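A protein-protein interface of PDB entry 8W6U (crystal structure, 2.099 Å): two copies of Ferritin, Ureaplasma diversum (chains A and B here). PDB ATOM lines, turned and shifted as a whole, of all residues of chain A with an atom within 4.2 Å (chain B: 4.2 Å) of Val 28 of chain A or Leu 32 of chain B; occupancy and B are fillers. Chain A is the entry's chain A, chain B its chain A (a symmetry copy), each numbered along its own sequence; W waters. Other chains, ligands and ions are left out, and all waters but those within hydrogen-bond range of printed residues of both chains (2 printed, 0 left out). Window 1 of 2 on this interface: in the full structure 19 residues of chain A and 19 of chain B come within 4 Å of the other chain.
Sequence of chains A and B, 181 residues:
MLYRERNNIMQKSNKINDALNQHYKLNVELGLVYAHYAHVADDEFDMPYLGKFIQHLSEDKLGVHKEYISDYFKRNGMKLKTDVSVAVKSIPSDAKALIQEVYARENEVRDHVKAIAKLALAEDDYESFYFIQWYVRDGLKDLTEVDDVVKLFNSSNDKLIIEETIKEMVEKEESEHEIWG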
ATOM      1  N   TYR A  24      12.890   6.191 -12.027  1.00  0.00           N
ATOM      2  CA  TYR A  24      12.518   4.776 -12.083  1.00  0.00           C
ATOM      3  C   TYR A  24      11.673   4.489 -13.319  1.00  0.00           C
ATOM      4  O   TYR A  24      11.940   3.545 -14.077  1.00  0.00           O
ATOM      5  CB  TYR A  24      11.761   4.419 -10.802  1.00  0.00           C
ATOM      6  CG  TYR A  24      11.315   2.971 -10.644  1.00  0.00           C
ATOM      7  CD1 TYR A  24      10.075   2.538 -11.133  1.00  0.00           C
ATOM      8  CD2 TYR A  24      12.109   2.053  -9.962  1.00  0.00           C
ATOM      9  CE1 TYR A  24       9.655   1.223 -10.966  1.00  0.00           C
ATOM     10  CE2 TYR A  24      11.704   0.734  -9.804  1.00  0.00           C
ATOM     11  CZ  TYR A  24      10.487   0.327 -10.306  1.00  0.00           C
ATOM     12  OH  TYR A  24      10.090  -0.978 -10.131  1.00  0.00           O
ATOM     13  N   LYS A  25      10.636   5.300 -13.520  1.00  0.00           N
ATOM     14  CA  LYS A  25       9.779   5.202 -14.694  1.00  0.00           C
ATOM     15  C   LYS A  25      10.584   5.328 -15.984  1.00  0.00           C
ATOM     16  O   LYS A  25      10.370   4.575 -16.943  1.00  0.00           O
ATOM     17  CB  LYS A  25       8.709   6.301 -14.598  1.00  0.00           C
ATOM     18  CG  LYS A  25       7.881   6.563 -15.845  1.00  0.00           C
ATOM     19  CD  LYS A  25       6.831   7.627 -15.539  1.00  0.00           C
ATOM     20  CE  LYS A  25       6.093   8.082 -16.787  1.00  0.00           C
ATOM     21  NZ  LYS A  25       5.166   7.021 -17.258  1.00  0.00           N
ATOM     22  N   LEU A  26      11.492   6.306 -16.039  1.00  0.00           N
ATOM     23  CA  LEU A  26      12.307   6.491 -17.238  1.00  0.00           C
ATOM     24  C   LEU A  26      13.122   5.231 -17.536  1.00  0.00           C
ATOM     25  O   LEU A  26      13.177   4.766 -18.682  1.00  0.00           O
ATOM     26  CB  LEU A  26      13.202   7.723 -17.046  1.00  0.00           C
ATOM     27  CG  LEU A  26      14.159   8.336 -18.085  1.00  0.00           C
ATOM     28  CD1 LEU A  26      15.536   7.733 -17.956  1.00  0.00           C
ATOM     29  CD2 LEU A  26      13.647   8.207 -19.514  1.00  0.00           C
ATOM     30  N   ASN A  27      13.714   4.626 -16.505  1.00  0.00           N
ATOM     31  CA  ASN A  27      14.548   3.448 -16.737  1.00  0.00           C
ATOM     32  C   ASN A  27      13.719   2.234 -17.151  1.00  0.00           C
ATOM     33  O   ASN A  27      14.156   1.433 -17.990  1.00  0.00           O
ATOM     34  CB  ASN A  27      15.370   3.152 -15.493  1.00  0.00           C
ATOM     35  CG  ASN A  27      16.649   3.944 -15.475  1.00  0.00           C
ATOM     36  OD1 ASN A  27      17.567   3.640 -16.225  1.00  0.00           O
ATOM     37  ND2 ASN A  27      16.699   4.997 -14.658  1.00  0.00           N
ATOM     38  N   VAL A  28      12.521   2.079 -16.587  1.00  0.00           N
ATOM     39  CA  VAL A  28      11.638   0.997 -17.031  1.00  0.00           C
ATOM     40  C   VAL A  28      11.283   1.178 -18.505  1.00  0.00           C
ATOM     41  O   VAL A  28      11.448   0.263 -19.325  1.00  0.00           O
ATOM     42  CB  VAL A  28      10.371   0.942 -16.157  1.00  0.00           C
ATOM     43  CG1 VAL A  28       9.286   0.122 -16.850  1.00  0.00           C
ATOM     44  CG2 VAL A  28      10.685   0.377 -14.778  1.00  0.00           C
ATOM     45  N   GLU A  29      10.812   2.376 -18.869  1.00  0.00           N
ATOM     46  CA  GLU A  29      10.323   2.603 -20.227  1.00  0.00           C
ATOM     47  C   GLU A  29      11.455   2.528 -21.247  1.00  0.00           C
ATOM     48  O   GLU A  29      11.303   1.897 -22.302  1.00  0.00           O
ATOM     49  CB  GLU A  29       9.580   3.948 -20.281  1.00  0.00           C
ATOM     50  CG  GLU A  29       8.277   3.849 -19.473  1.00  0.00           C
ATOM     51  CD  GLU A  29       7.493   5.150 -19.317  1.00  0.00           C
ATOM     52  OE1 GLU A  29       6.394   5.064 -18.737  1.00  0.00           O
ATOM     53  OE2 GLU A  29       7.953   6.235 -19.739  1.00  0.00           O
ATOM     54  N   LEU A  30      12.603   3.133 -20.934  1.00  0.00           N
ATOM     55  CA  LEU A  30      13.794   2.989 -21.769  1.00  0.00           C
ATOM     56  C   LEU A  30      14.131   1.520 -22.017  1.00  0.00           C
ATOM     57  O   LEU A  30      14.393   1.109 -23.159  1.00  0.00           O
ATOM     58  CB  LEU A  30      14.983   3.683 -21.100  1.00  0.00           C
ATOM     59  CG  LEU A  30      15.519   4.989 -21.663  1.00  0.00           C
ATOM     60  CD1 LEU A  30      16.852   5.310 -20.989  1.00  0.00           C
ATOM     61  CD2 LEU A  30      15.663   4.905 -23.170  1.00  0.00           C
ATOM     62  N   GLY A  31      14.136   0.718 -20.950  1.00  0.00           N
ATOM     63  CA  GLY A  31      14.477  -0.691 -21.086  1.00  0.00           C
ATOM     64  C   GLY A  31      13.525  -1.438 -21.997  1.00  0.00           C
ATOM     65  O   GLY A  31      13.936  -2.327 -22.749  1.00  0.00           O
ATOM     66  N   LEU A  32      12.242  -1.083 -21.951  1.00  0.00           N
ATOM     67  CA  LEU A  32      11.263  -1.722 -22.825  1.00  0.00           C
ATOM     68  C   LEU A  32      11.454  -1.293 -24.276  1.00  0.00           C
ATOM     69  O   LEU A  32      11.323  -2.112 -25.200  1.00  0.00           O
ATOM     70  CB  LEU A  32       9.852  -1.399 -22.333  1.00  0.00           C
ATOM     71  CG  LEU A  32       9.507  -2.086 -21.005  1.00  0.00           C
ATOM     72  CD1 LEU A  32       8.169  -1.622 -20.441  1.00  0.00           C
ATOM     73  CD2 LEU A  32       9.520  -3.598 -21.184  1.00  0.00           C
ATOM     74  N   LEU A  62      16.468  -2.051 -16.871  1.00  0.00           N
ATOM     75  CA  LEU A  62      15.416  -2.738 -16.173  1.00  0.00           C
ATOM     76  C   LEU A  62      15.925  -3.562 -15.021  1.00  0.00           C
ATOM     77  O   LEU A  62      15.161  -4.175 -14.328  1.00  0.00           O
ATOM     78  CB  LEU A  62      14.648  -3.589 -17.161  1.00  0.00           C
ATOM     79  CG  LEU A  62      13.569  -2.990 -18.047  1.00  0.00           C
ATOM     80  CD1 LEU A  62      13.362  -3.903 -19.237  1.00  0.00           C
ATOM     81  CD2 LEU A  62      12.287  -2.862 -17.256  1.00  0.00           C
ATOM     82  N   LYS A  66      16.859   0.391 -11.988  1.00  0.00           N
ATOM     83  CA  LYS A  66      15.628   0.466 -11.231  1.00  0.00           C
ATOM     84  C   LYS A  66      15.715  -0.138  -9.845  1.00  0.00           C
ATOM     85  O   LYS A  66      15.139   0.374  -8.914  1.00  0.00           O
ATOM     86  CB  LYS A  66      14.473  -0.106 -12.031  1.00  0.00           C
ATOM     87  CG  LYS A  66      14.164  -1.587 -11.915  1.00  0.00           C
ATOM     88  CD  LYS A  66      12.930  -1.931 -12.719  1.00  0.00           C
ATOM     89  CE  LYS A  66      12.312  -3.242 -12.280  1.00  0.00           C
ATOM     90  NZ  LYS A  66      13.329  -4.291 -12.054  1.00  0.00           N
ATOM     91  N   VAL A  84       3.601   3.098 -15.684  1.00  0.00           N
ATOM     92  CA  VAL A  84       4.319   2.944 -16.916  1.00  0.00           C
ATOM     93  C   VAL A  84       3.471   3.038 -18.149  1.00  0.00           C
ATOM     94  O   VAL A  84       2.442   2.417 -18.221  1.00  0.00           O
ATOM     95  CB  VAL A  84       5.074   1.583 -16.906  1.00  0.00           C
ATOM     96  CG1 VAL A  84       5.816   1.309 -18.196  1.00  0.00           C
ATOM     97  CG2 VAL A  84       6.007   1.491 -15.713  1.00  0.00           C
ATOM     98  N   VAL B  28       5.265  -8.599 -19.729  1.00  0.00           N
ATOM     99  CA  VAL B  28       5.928  -7.349 -19.345  1.00  0.00           C
ATOM    100  C   VAL B  28       5.197  -6.705 -18.170  1.00  0.00           C
ATOM    101  O   VAL B  28       5.800  -6.374 -17.139  1.00  0.00           O
ATOM    102  CB  VAL B  28       6.004  -6.389 -20.547  1.00  0.00           C
ATOM    103  CG1 VAL B  28       6.301  -4.969 -20.071  1.00  0.00           C
ATOM    104  CG2 VAL B  28       7.048  -6.856 -21.553  1.00  0.00           C
ATOM    105  N   GLU B  29       3.876  -6.540 -18.299  1.00  0.00           N
ATOM    106  CA  GLU B  29       3.113  -5.815 -17.285  1.00  0.00           C
ATOM    107  C   GLU B  29       3.080  -6.575 -15.962  1.00  0.00           C
ATOM    108  O   GLU B  29       3.277  -5.979 -14.895  1.00  0.00           O
ATOM    109  CB  GLU B  29       1.703  -5.523 -17.822  1.00  0.00           C
ATOM    110  CG  GLU B  29       1.790  -4.499 -18.965  1.00  0.00           C
ATOM    111  CD  GLU B  29       0.481  -4.209 -19.696  1.00  0.00           C
ATOM    112  OE1 GLU B  29       0.522  -3.319 -20.567  1.00  0.00           O
ATOM    113  OE2 GLU B  29      -0.561  -4.851 -19.434  1.00  0.00           O
ATOM    114  N   LEU B  30       2.868  -7.892 -16.018  1.00  0.00           N
ATOM    115  CA  LEU B  30       2.972  -8.734 -14.827  1.00  0.00           C
ATOM    116  C   LEU B  30       4.311  -8.539 -14.118  1.00  0.00           C
ATOM    117  O   LEU B  30       4.364  -8.367 -12.891  1.00  0.00           O
ATOM    118  CB  LEU B  30       2.805 -10.204 -15.215  1.00  0.00           C
ATOM    119  CG  LEU B  30       1.530 -10.948 -14.855  1.00  0.00           C
ATOM    120  CD1 LEU B  30       1.738 -12.441 -15.106  1.00  0.00           C
ATOM    121  CD2 LEU B  30       1.136 -10.674 -13.417  1.00  0.00           C
ATOM    122  N   GLY B  31       5.405  -8.572 -14.884  1.00  0.00           N
ATOM    123  CA  GLY B  31       6.727  -8.427 -14.291  1.00  0.00           C
ATOM    124  C   GLY B  31       6.912  -7.096 -13.591  1.00  0.00           C
ATOM    125  O   GLY B  31       7.564  -7.018 -12.546  1.00  0.00           O
ATOM    126  N   LEU B  32       6.331  -6.035 -14.149  1.00  0.00           N
ATOM    127  CA  LEU B  32       6.424  -4.722 -13.519  1.00  0.00           C
ATOM    128  C   LEU B  32       5.586  -4.660 -12.245  1.00  0.00           C
ATOM    129  O   LEU B  32       6.005  -4.059 -11.242  1.00  0.00           O
ATOM    130  CB  LEU B  32       5.995  -3.646 -14.516  1.00  0.00           C
ATOM    131  CG  LEU B  32       6.995  -3.458 -15.664  1.00  0.00           C
ATOM    132  CD1 LEU B  32       6.476  -2.509 -16.739  1.00  0.00           C
ATOM    133  CD2 LEU B  32       8.329  -2.970 -15.114  1.00  0.00           C
ATOM    134  N   VAL B  33       4.406  -5.283 -12.261  1.00  0.00           N
ATOM    135  CA  VAL B  33       3.585  -5.357 -11.056  1.00  0.00           C
ATOM    136  C   VAL B  33       4.306  -6.160  -9.980  1.00  0.00           C
ATOM    137  O   VAL B  33       4.357  -5.767  -8.808  1.00  0.00           O
ATOM    138  CB  VAL B  33       2.205  -5.960 -11.377  1.00  0.00           C
ATOM    139  CG1 VAL B  33       1.425  -6.234 -10.097  1.00  0.00           C
ATOM    140  CG2 VAL B  33       1.411  -5.025 -12.280  1.00  0.00           C
ATOM    141  N   TYR B  34       4.866  -7.304 -10.367  1.00  0.00           N
ATOM    142  CA  TYR B  34       5.558  -8.150  -9.402  1.00  0.00           C
ATOM    143  C   TYR B  34       6.758  -7.426  -8.797  1.00  0.00           C
ATOM    144  O   TYR B  34       7.033  -7.569  -7.601  1.00  0.00           O
ATOM    145  CB  TYR B  34       5.987  -9.460 -10.068  1.00  0.00           C
ATOM    146  CG  TYR B  34       4.859 -10.414 -10.375  1.00  0.00           C
ATOM    147  CD1 TYR B  34       3.582 -10.205  -9.876  1.00  0.00           C
ATOM    148  CD2 TYR B  34       5.080 -11.540 -11.153  1.00  0.00           C
ATOM    149  CE1 TYR B  34       2.550 -11.081 -10.158  1.00  0.00           C
ATOM    150  CE2 TYR B  34       4.058 -12.427 -11.430  1.00  0.00           C
ATOM    151  CZ  TYR B  34       2.796 -12.198 -10.925  1.00  0.00           C
ATOM    152  OH  TYR B  34       1.776 -13.080 -11.214  1.00  0.00           O
ATOM    153  N   ALA B  35       7.479  -6.634  -9.601  1.00  0.00           N
ATOM    154  CA  ALA B  35       8.582  -5.853  -9.050  1.00  0.00           C
ATOM    155  C   ALA B  35       8.083  -4.912  -7.957  1.00  0.00           C
ATOM    156  O   ALA B  35       8.729  -4.757  -6.914  1.00  0.00           O
ATOM    157  CB  ALA B  35       9.291  -5.060 -10.152  1.00  0.00           C
ATOM    158  N   HIS B  36       6.926  -4.287  -8.174  1.00  0.00           N
ATOM    159  CA  HIS B  36       6.332  -3.443  -7.142  1.00  0.00           C
ATOM    160  C   HIS B  36       5.931  -4.271  -5.928  1.00  0.00           C
ATOM    161  O   HIS B  36       6.261  -3.919  -4.790  1.00  0.00           O
ATOM    162  CB  HIS B  36       5.126  -2.701  -7.704  1.00  0.00           C
ATOM    163  CG  HIS B  36       4.741  -1.489  -6.914  1.00  0.00           C
ATOM    164  ND1 HIS B  36       4.150  -1.566  -5.671  1.00  0.00           N
ATOM    165  CD2 HIS B  36       4.843  -0.171  -7.202  1.00  0.00           C
ATOM    166  CE1 HIS B  36       3.926  -0.344  -5.216  1.00  0.00           C
ATOM    167  NE2 HIS B  36       4.339   0.520  -6.127  1.00  0.00           N
ATOM    168  N   LEU B  62       9.795 -10.914 -17.114  1.00  0.00           N
ATOM    169  CA  LEU B  62      10.439  -9.917 -17.925  1.00  0.00           C
ATOM    170  C   LEU B  62      11.686 -10.429 -18.594  1.00  0.00           C
ATOM    171  O   LEU B  62      12.320  -9.717 -19.323  1.00  0.00           O
ATOM    172  CB  LEU B  62      10.732  -8.705 -17.068  1.00  0.00           C
ATOM    173  CG  LEU B  62       9.661  -7.669 -16.772  1.00  0.00           C
ATOM    174  CD1 LEU B  62      10.061  -6.903 -15.530  1.00  0.00           C
ATOM    175  CD2 LEU B  62       9.538  -6.729 -17.950  1.00  0.00           C
ATOM    176  N   VAL B  86       0.750   0.071 -17.509  1.00  0.00           N
ATOM    177  CA  VAL B  86       0.536  -0.489 -16.211  1.00  0.00           C
ATOM    178  C   VAL B  86       0.693   0.507 -15.074  1.00  0.00           C
ATOM    179  O   VAL B  86       1.602   1.310 -15.074  1.00  0.00           O
ATOM    180  CB  VAL B  86       1.383  -1.775 -15.982  1.00  0.00           C
ATOM    181  CG1 VAL B  86       2.865  -1.510 -15.856  1.00  0.00           C
ATOM    182  CG2 VAL B  86       0.834  -2.588 -14.833  1.00  0.00           C
HETATM  183  O   HOH W   1       7.553  -1.682 -10.763  1.00  0.00           O
HETATM  184  O   HOH W   2       0.242   3.841 -16.700  1.00  0.00           O
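N of Val 84 of chain A is in hydrogen-bond range of O of Val 86 of chain B (2.8 Å).
Among the printed residues, pairs that only touch across the chains: Val 28 of chain A with Leu 32 of chain B (3.7 Å) and Leu 32 of chain A with Val 28 of chain B (3.7 Å).
Tyr 24 of chain A touches none of the printed residues of chain B. Printed residues of chain B within 4 Å of Leu 32 of chain A: Val 28 (3.7 Å). Printed residues of chain B within 4 Å of Val 84 of chain A: Val 86. Of the printed residues of chain A, Val 28 of chain B touches Leu 32. Leu 32 of chain B touches one residue of chain A. Leu 62 of chain B touches none of the printed residues of chain A. Printed residues of chain A within 4 Å of Val 86 of chain B: Val 84 (2.8 Å).
Hydrophobic or aromatic side chains of chain A that line the printed part of chain B: Val 28, Leu 32 and Val 84. Among the printed residues, 3 pairs touch across the chains.
Val 28 of chain A touches Leu 32 of chain B, and with the chains exchanged Leu 32 of chain A touches Val 28 of chain B. Of the 3 pairs that touch across the chains among the printed residues, 2 have their exchanged pair printed and touching as well.
Water W1 bridges OH of Tyr 24 of chain A (2.7 Å) and O of Leu 32 of chain B (2.9 Å). Water W2 bridges the backbone carbonyl oxygen of Val 84 of chain A (3.0 Å) and the backbone carbonyl oxygen of Val 86 of chain B (3.3 Å).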
